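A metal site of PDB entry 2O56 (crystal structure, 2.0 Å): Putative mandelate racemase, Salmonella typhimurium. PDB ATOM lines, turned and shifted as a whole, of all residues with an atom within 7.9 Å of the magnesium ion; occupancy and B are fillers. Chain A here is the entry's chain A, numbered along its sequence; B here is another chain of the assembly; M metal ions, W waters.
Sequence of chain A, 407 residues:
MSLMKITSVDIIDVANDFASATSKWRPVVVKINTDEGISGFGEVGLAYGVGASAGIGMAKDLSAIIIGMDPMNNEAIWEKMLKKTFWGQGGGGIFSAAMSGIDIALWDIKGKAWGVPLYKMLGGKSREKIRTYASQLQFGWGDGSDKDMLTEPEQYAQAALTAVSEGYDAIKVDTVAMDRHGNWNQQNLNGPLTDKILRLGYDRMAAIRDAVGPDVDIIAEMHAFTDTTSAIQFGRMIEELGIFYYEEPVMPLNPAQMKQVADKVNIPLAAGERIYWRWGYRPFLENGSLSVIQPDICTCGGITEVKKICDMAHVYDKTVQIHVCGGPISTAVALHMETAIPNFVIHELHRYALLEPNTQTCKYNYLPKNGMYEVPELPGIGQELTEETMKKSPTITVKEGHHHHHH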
ATOM      1  N   TYR A  48      15.137 -25.282  -2.820  1.00  0.00           N
ATOM      2  CA  TYR A  48      14.916 -24.041  -2.070  1.00  0.00           C
ATOM      3  C   TYR A  48      13.485 -24.101  -1.564  1.00  0.00           C
ATOM      4  O   TYR A  48      12.755 -25.063  -1.845  1.00  0.00           O
ATOM      5  CB  TYR A  48      15.102 -22.827  -2.983  1.00  0.00           C
ATOM      6  CG  TYR A  48      14.312 -22.975  -4.246  1.00  0.00           C
ATOM      7  CD1 TYR A  48      13.039 -22.441  -4.365  1.00  0.00           C
ATOM      8  CD2 TYR A  48      14.812 -23.715  -5.313  1.00  0.00           C
ATOM      9  CE1 TYR A  48      12.294 -22.623  -5.507  1.00  0.00           C
ATOM     10  CE2 TYR A  48      14.077 -23.911  -6.451  1.00  0.00           C
ATOM     11  CZ  TYR A  48      12.821 -23.365  -6.545  1.00  0.00           C
ATOM     12  OH  TYR A  48      12.090 -23.553  -7.687  1.00  0.00           O
ATOM     13  N   TYR A 133      18.836 -16.238 -20.613  1.00  0.00           N
ATOM     14  CA  TYR A 133      18.844 -14.982 -19.859  1.00  0.00           C
ATOM     15  C   TYR A 133      19.564 -15.099 -18.519  1.00  0.00           C
ATOM     16  O   TYR A 133      19.667 -16.186 -17.955  1.00  0.00           O
ATOM     17  CB  TYR A 133      17.434 -14.393 -19.704  1.00  0.00           C
ATOM     18  CG  TYR A 133      16.441 -15.138 -18.833  1.00  0.00           C
ATOM     19  CD1 TYR A 133      16.446 -14.988 -17.442  1.00  0.00           C
ATOM     20  CD2 TYR A 133      15.455 -15.938 -19.398  1.00  0.00           C
ATOM     21  CE1 TYR A 133      15.503 -15.660 -16.628  1.00  0.00           C
ATOM     22  CE2 TYR A 133      14.512 -16.615 -18.597  1.00  0.00           C
ATOM     23  CZ  TYR A 133      14.544 -16.458 -17.218  1.00  0.00           C
ATOM     24  OH  TYR A 133      13.620 -17.104 -16.405  1.00  0.00           O
ATOM     25  N   SER A 135      19.365 -14.604 -14.806  1.00  0.00           N
ATOM     26  CA  SER A 135      18.160 -14.661 -13.949  1.00  0.00           C
ATOM     27  C   SER A 135      18.441 -14.052 -12.571  1.00  0.00           C
ATOM     28  O   SER A 135      19.531 -14.227 -12.031  1.00  0.00           O
ATOM     29  CB  SER A 135      17.699 -16.108 -13.771  1.00  0.00           C
ATOM     30  OG  SER A 135      16.384 -16.171 -13.197  1.00  0.00           O
ATOM     31  N   GLN A 136      17.453 -13.349 -12.023  1.00  0.00           N
ATOM     32  CA  GLN A 136      17.462 -12.805 -10.652  1.00  0.00           C
ATOM     33  C   GLN A 136      18.553 -11.779 -10.325  1.00  0.00           C
ATOM     34  O   GLN A 136      19.295 -11.929  -9.340  1.00  0.00           O
ATOM     35  CB  GLN A 136      17.357 -13.908  -9.586  1.00  0.00           C
ATOM     36  CG  GLN A 136      16.366 -15.058  -9.879  1.00  0.00           C
ATOM     37  CD  GLN A 136      14.870 -14.660  -9.850  1.00  0.00           C
ATOM     38  OE1 GLN A 136      14.507 -13.491  -9.702  1.00  0.00           O
ATOM     39  NE2 GLN A 136      13.999 -15.657  -9.984  1.00  0.00           N
ATOM     40  N   LYS A 172      16.333 -11.271 -16.229  1.00  0.00           N
ATOM     41  CA  LYS A 172      15.151 -11.235 -15.374  1.00  0.00           C
ATOM     42  C   LYS A 172      15.451 -10.708 -13.977  1.00  0.00           C
ATOM     43  O   LYS A 172      16.529 -10.945 -13.431  1.00  0.00           O
ATOM     44  CB  LYS A 172      14.548 -12.632 -15.264  1.00  0.00           C
ATOM     45  CG  LYS A 172      13.332 -12.697 -14.314  1.00  0.00           C
ATOM     46  CD  LYS A 172      12.716 -14.083 -14.386  1.00  0.00           C
ATOM     47  CE  LYS A 172      13.262 -15.004 -13.321  1.00  0.00           C
ATOM     48  NZ  LYS A 172      12.684 -16.393 -13.580  1.00  0.00           N
ATOM     49  N   GLU A 221       9.920 -10.422 -12.730  1.00  0.00           N
ATOM     50  CA  GLU A 221       9.594 -11.585 -11.915  1.00  0.00           C
ATOM     51  C   GLU A 221       8.962 -11.086 -10.626  1.00  0.00           C
ATOM     52  O   GLU A 221       9.422 -10.105 -10.046  1.00  0.00           O
ATOM     53  CB  GLU A 221      10.892 -12.368 -11.656  1.00  0.00           C
ATOM     54  CG  GLU A 221      10.982 -13.126 -10.380  1.00  0.00           C
ATOM     55  CD  GLU A 221      10.369 -14.512 -10.481  1.00  0.00           C
ATOM     56  OE1 GLU A 221      11.118 -15.485 -10.695  1.00  0.00           O
ATOM     57  OE2 GLU A 221       9.132 -14.617 -10.345  1.00  0.00           O
ATOM     58  N   MET A 222       7.880 -11.740 -10.190  1.00  0.00           N
ATOM     59  CA  MET A 222       7.127 -11.277  -9.025  1.00  0.00           C
ATOM     60  C   MET A 222       7.092 -12.313  -7.910  1.00  0.00           C
ATOM     61  O   MET A 222       6.709 -11.984  -6.789  1.00  0.00           O
ATOM     62  CB  MET A 222       5.687 -10.938  -9.412  1.00  0.00           C
ATOM     63  CG  MET A 222       5.515  -9.824 -10.406  1.00  0.00           C
ATOM     64  SD  MET A 222       6.383  -8.298  -9.985  1.00  0.00           S
ATOM     65  CE  MET A 222       5.265  -7.567  -8.812  1.00  0.00           C
ATOM     66  N   HIS A 223       7.430 -13.561  -8.247  1.00  0.00           N
ATOM     67  CA  HIS A 223       7.549 -14.662  -7.284  1.00  0.00           C
ATOM     68  C   HIS A 223       6.219 -15.056  -6.622  1.00  0.00           C
ATOM     69  O   HIS A 223       6.231 -15.822  -5.659  1.00  0.00           O
ATOM     70  CB  HIS A 223       8.552 -14.342  -6.173  1.00  0.00           C
ATOM     71  CG  HIS A 223       9.990 -14.435  -6.583  1.00  0.00           C
ATOM     72  ND1 HIS A 223      10.794 -13.327  -6.766  1.00  0.00           N
ATOM     73  CD2 HIS A 223      10.781 -15.514  -6.815  1.00  0.00           C
ATOM     74  CE1 HIS A 223      12.006 -13.709  -7.105  1.00  0.00           C
ATOM     75  NE2 HIS A 223      12.028 -15.034  -7.144  1.00  0.00           N
ATOM     76  N   ALA A 224       5.094 -14.515  -7.116  1.00  0.00           N
ATOM     77  CA  ALA A 224       3.791 -14.588  -6.457  1.00  0.00           C
ATOM     78  C   ALA A 224       3.800 -14.066  -5.019  1.00  0.00           C
ATOM     79  O   ALA A 224       3.077 -14.588  -4.155  1.00  0.00           O
ATOM     80  CB  ALA A 224       3.215 -16.026  -6.529  1.00  0.00           C
ATOM     81  N   GLU A 247       6.294 -12.521 -14.861  1.00  0.00           N
ATOM     82  CA  GLU A 247       6.381 -13.898 -14.357  1.00  0.00           C
ATOM     83  C   GLU A 247       5.737 -14.075 -12.978  1.00  0.00           C
ATOM     84  O   GLU A 247       6.010 -13.313 -12.052  1.00  0.00           O
ATOM     85  CB  GLU A 247       7.855 -14.389 -14.317  1.00  0.00           C
ATOM     86  CG  GLU A 247       8.009 -15.739 -13.654  1.00  0.00           C
ATOM     87  CD  GLU A 247       9.403 -16.322 -13.750  1.00  0.00           C
ATOM     88  OE1 GLU A 247      10.157 -15.978 -14.684  1.00  0.00           O
ATOM     89  OE2 GLU A 247       9.733 -17.134 -12.873  1.00  0.00           O
ATOM     90  N   GLU A 248       4.887 -15.082 -12.856  1.00  0.00           N
ATOM     91  CA  GLU A 248       4.184 -15.371 -11.607  1.00  0.00           C
ATOM     92  C   GLU A 248       3.609 -14.155 -10.881  1.00  0.00           C
ATOM     93  O   GLU A 248       3.892 -13.949  -9.697  1.00  0.00           O
ATOM     94  CB  GLU A 248       5.122 -16.127 -10.657  1.00  0.00           C
ATOM     95  CG  GLU A 248       5.363 -17.583 -11.053  1.00  0.00           C
ATOM     96  CD  GLU A 248       5.706 -18.454  -9.874  1.00  0.00           C
ATOM     97  OE1 GLU A 248       6.761 -18.200  -9.273  1.00  0.00           O
ATOM     98  OE2 GLU A 248       4.926 -19.384  -9.550  1.00  0.00           O
ATOM     99  N   ALA A 270       3.732 -15.127 -17.668  1.00  0.00           N
ATOM    100  CA  ALA A 270       4.376 -16.424 -17.566  1.00  0.00           C
ATOM    101  C   ALA A 270       4.164 -17.021 -16.185  1.00  0.00           C
ATOM    102  O   ALA A 270       4.098 -16.302 -15.188  1.00  0.00           O
ATOM    103  CB  ALA A 270       5.863 -16.323 -17.887  1.00  0.00           C
ATOM    104  N   ALA A 271       4.035 -18.339 -16.135  1.00  0.00           N
ATOM    105  CA  ALA A 271       3.965 -19.041 -14.869  1.00  0.00           C
ATOM    106  C   ALA A 271       4.216 -20.480 -15.204  1.00  0.00           C
ATOM    107  O   ALA A 271       4.149 -20.867 -16.370  1.00  0.00           O
ATOM    108  CB  ALA A 271       2.578 -18.874 -14.225  1.00  0.00           C
ATOM    109  N   GLY A 272       4.493 -21.278 -14.164  1.00  0.00           N
ATOM    110  CA  GLY A 272       4.544 -22.726 -14.351  1.00  0.00           C
ATOM    111  C   GLY A 272       5.411 -23.477 -13.347  1.00  0.00           C
ATOM    112  O   GLY A 272       5.252 -24.676 -13.164  1.00  0.00           O
ATOM    113  N   GLU A 273       6.323 -22.778 -12.676  1.00  0.00           N
ATOM    114  CA  GLU A 273       7.167 -23.478 -11.687  1.00  0.00           C
ATOM    115  C   GLU A 273       6.345 -24.113 -10.556  1.00  0.00           C
ATOM    116  O   GLU A 273       6.790 -25.103  -9.940  1.00  0.00           O
ATOM    117  CB  GLU A 273       8.278 -22.583 -11.153  1.00  0.00           C
ATOM    118  CG  GLU A 273       7.843 -21.385 -10.338  1.00  0.00           C
ATOM    119  CD  GLU A 273       8.966 -20.389 -10.182  1.00  0.00           C
ATOM    120  OE1 GLU A 273       9.075 -19.474 -11.029  1.00  0.00           O
ATOM    121  OE2 GLU A 273       9.758 -20.515  -9.231  1.00  0.00           O
ATOM    122  N   ARG A 274       5.162 -23.567 -10.303  1.00  0.00           N
ATOM    123  CA  ARG A 274       4.253 -24.084  -9.303  1.00  0.00           C
ATOM    124  C   ARG A 274       2.916 -24.577  -9.830  1.00  0.00           C
ATOM    125  O   ARG A 274       1.943 -24.655  -9.099  1.00  0.00           O
ATOM    126  CB  ARG A 274       4.079 -23.084  -8.170  1.00  0.00           C
ATOM    127  CG  ARG A 274       5.294 -23.030  -7.251  1.00  0.00           C
ATOM    128  CD  ARG A 274       5.100 -21.984  -6.206  1.00  0.00           C
ATOM    129  NE  ARG A 274       5.400 -20.660  -6.737  1.00  0.00           N
ATOM    130  CZ  ARG A 274       5.585 -19.588  -5.984  1.00  0.00           C
ATOM    131  NH1 ARG A 274       5.485 -19.704  -4.664  1.00  0.00           N
ATOM    132  NH2 ARG A 274       5.877 -18.416  -6.532  1.00  0.00           N
ATOM    133  N   GLN A 294       6.241 -22.232 -17.851  1.00  0.00           N
ATOM    134  CA  GLN A 294       7.535 -22.435 -17.232  1.00  0.00           C
ATOM    135  C   GLN A 294       7.606 -23.668 -16.342  1.00  0.00           C
ATOM    136  O   GLN A 294       8.008 -23.547 -15.182  1.00  0.00           O
ATOM    137  CB  GLN A 294       7.954 -21.213 -16.416  1.00  0.00           C
ATOM    138  CG  GLN A 294       7.811 -19.895 -17.188  1.00  0.00           C
ATOM    139  CD  GLN A 294       8.046 -18.695 -16.309  1.00  0.00           C
ATOM    140  OE1 GLN A 294       7.365 -18.502 -15.326  1.00  0.00           O
ATOM    141  NE2 GLN A 294       9.041 -17.901 -16.652  1.00  0.00           N
ATOM    142  N   GLN A 321       9.607 -21.615 -21.511  1.00  0.00           N
ATOM    143  CA  GLN A 321      10.877 -21.422 -20.843  1.00  0.00           C
ATOM    144  C   GLN A 321      10.898 -22.363 -19.652  1.00  0.00           C
ATOM    145  O   GLN A 321      10.243 -22.087 -18.661  1.00  0.00           O
ATOM    146  CB  GLN A 321      10.978 -19.971 -20.330  1.00  0.00           C
ATOM    147  CG  GLN A 321      12.241 -19.741 -19.472  1.00  0.00           C
ATOM    148  CD  GLN A 321      11.949 -19.181 -18.105  1.00  0.00           C
ATOM    149  OE1 GLN A 321      11.545 -18.018 -17.960  1.00  0.00           O
ATOM    150  NE2 GLN A 321      12.185 -19.990 -17.081  1.00  0.00           N
ATOM    151  N   HIS A 323      11.580 -23.824 -16.259  1.00  0.00           N
ATOM    152  CA  HIS A 323      12.075 -23.292 -14.994  1.00  0.00           C
ATOM    153  C   HIS A 323      13.270 -24.116 -14.529  1.00  0.00           C
ATOM    154  O   HIS A 323      13.172 -25.328 -14.405  1.00  0.00           O
ATOM    155  CB  HIS A 323      10.999 -23.291 -13.911  1.00  0.00           C
ATOM    156  CG  HIS A 323      11.518 -22.891 -12.566  1.00  0.00           C
ATOM    157  ND1 HIS A 323      11.954 -23.808 -11.630  1.00  0.00           N
ATOM    158  CD2 HIS A 323      11.754 -21.665 -12.031  1.00  0.00           C
ATOM    159  CE1 HIS A 323      12.397 -23.166 -10.571  1.00  0.00           C
ATOM    160  NE2 HIS A 323      12.284 -21.867 -10.779  1.00  0.00           N
ATOM    161  N   VAL A 324      14.404 -23.465 -14.296  1.00  0.00           N
ATOM    162  CA  VAL A 324      15.585 -24.154 -13.822  1.00  0.00           C
ATOM    163  C   VAL A 324      16.138 -23.469 -12.574  1.00  0.00           C
ATOM    164  O   VAL A 324      16.640 -22.348 -12.647  1.00  0.00           O
ATOM    165  CB  VAL A 324      16.707 -24.230 -14.899  1.00  0.00           C
ATOM    166  CG1 VAL A 324      17.913 -25.014 -14.373  1.00  0.00           C
ATOM    167  CG2 VAL A 324      16.211 -24.892 -16.173  1.00  0.00           C
ATOM    168  N   CYS A 325      16.045 -24.161 -11.437  1.00  0.00           N
ATOM    169  CA  CYS A 325      16.752 -23.738 -10.215  1.00  0.00           C
ATOM    170  C   CYS A 325      17.165 -24.950  -9.389  1.00  0.00           C
ATOM    171  O   CYS A 325      16.604 -25.227  -8.317  1.00  0.00           O
ATOM    172  CB  CYS A 325      15.875 -22.787  -9.383  1.00  0.00           C
ATOM    173  SG  CYS A 325      16.795 -21.842  -8.108  1.00  0.00           S
ATOM    174  N   GLU A 348      16.614 -20.221 -18.671  1.00  0.00           N
ATOM    175  CA  GLU A 348      16.900 -19.464 -17.454  1.00  0.00           C
ATOM    176  C   GLU A 348      18.256 -19.819 -16.862  1.00  0.00           C
ATOM    177  O   GLU A 348      18.501 -20.970 -16.495  1.00  0.00           O
ATOM    178  CB  GLU A 348      15.821 -19.731 -16.385  1.00  0.00           C
ATOM    179  CG  GLU A 348      16.093 -19.058 -15.035  1.00  0.00           C
ATOM    180  CD  GLU A 348      14.925 -19.167 -14.051  1.00  0.00           C
ATOM    181  OE1 GLU A 348      14.154 -20.139 -14.154  1.00  0.00           O
ATOM    182  OE2 GLU A 348      14.794 -18.277 -13.174  1.00  0.00           O
ATOM    183  N   HIS A 350      20.737 -19.013 -13.654  1.00  0.00           N
ATOM    184  CA  HIS A 350      21.119 -18.389 -12.399  1.00  0.00           C
ATOM    185  C   HIS A 350      22.622 -18.316 -12.294  1.00  0.00           C
ATOM    186  O   HIS A 350      23.335 -19.178 -12.825  1.00  0.00           O
ATOM    187  CB  HIS A 350      20.619 -19.181 -11.212  1.00  0.00           C
ATOM    188  CG  HIS A 350      19.132 -19.291 -11.142  1.00  0.00           C
ATOM    189  ND1 HIS A 350      18.366 -18.437 -10.381  1.00  0.00           N
ATOM    190  CD2 HIS A 350      18.275 -20.154 -11.723  1.00  0.00           C
ATOM    191  CE1 HIS A 350      17.091 -18.773 -10.487  1.00  0.00           C
ATOM    192  NE2 HIS A 350      17.012 -19.822 -11.298  1.00  0.00           N
ATOM    193  N   PHE B  86       7.145 -21.071  -0.151  1.00  0.00           N
ATOM    194  CA  PHE B  86       7.220 -21.244  -1.605  1.00  0.00           C
ATOM    195  C   PHE B  86       6.286 -22.291  -2.181  1.00  0.00           C
ATOM    196  O   PHE B  86       5.415 -21.975  -2.989  1.00  0.00           O
ATOM    197  CB  PHE B  86       8.657 -21.419  -2.145  1.00  0.00           C
ATOM    198  CG  PHE B  86       8.805 -21.041  -3.577  1.00  0.00           C
ATOM    199  CD1 PHE B  86       9.022 -19.699  -3.930  1.00  0.00           C
ATOM    200  CD2 PHE B  86       8.689 -21.994  -4.582  1.00  0.00           C
ATOM    201  CE1 PHE B  86       9.125 -19.336  -5.265  1.00  0.00           C
ATOM    202  CE2 PHE B  86       8.792 -21.635  -5.931  1.00  0.00           C
ATOM    203  CZ  PHE B  86       9.006 -20.297  -6.268  1.00  0.00           C
HETATM  204 MG    MG M   1      10.507 -17.737 -10.897  1.00  0.00          MG
HETATM  205  O   HOH W   1       8.583 -16.846  -9.761  1.00  0.00           O
HETATM  206  O   HOH W   2      12.511 -18.633 -11.238  1.00  0.00           O
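The magnesium ion is bound by the side-chain carboxylate of Glu 247 (2.2 Å), water W2 (2.2 Å), the side-chain carboxylate of Glu 273 (2.3 Å), the side-chain carboxylate of Glu 221 (2.3 Å) and water W1 (2.4 Å). The magnesium ion has five donor atoms within binding distance.
Water W2 lies within hydrogen-bond range of OE2 of Glu 348 (3.0 Å), NZ of Lys 172 (3.2 Å) and NE2 of His 323 (3.3 Å).
Lys 172 touches the magnesium ion. Within 4 Å of the magnesium ion: Lys 172, Glu 221, Glu 247 and Glu 273.
NZ of Lys 172 lies close to OE1 of Glu 221 (3.4 Å). The backbone NH (N) of Met 222 lies within hydrogen-bond range of the backbone carbonyl oxygen (O) of Glu 247. OH of Tyr 133 lies within hydrogen-bond range of NZ of Lys 172, at 3.1 Å. The backbone carbonyl oxygen (O) of Lys 172 is in hydrogen-bond range of the backbone NH (N) of Gln 136, at 2.9 Å. The side-chain amino group (NZ) of Lys 172 lies within salt-bridge range of the side-chain carboxylate (OE2) of Glu 348, at 2.9 Å. The side-chain carboxylate (OE1) of Glu 247 sits at hydrogen-bond distance from the side-chain amide nitrogen (NE2) of Gln 294, at 3.0 Å. NZ of Lys 172 lies within salt-bridge range of OE1 of Glu 247, 2.8 Å away. The side-chain carboxylate (OE2) of Glu 221 sits at hydrogen-bond distance from the backbone NH (N) of His 223 (2.9 Å).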
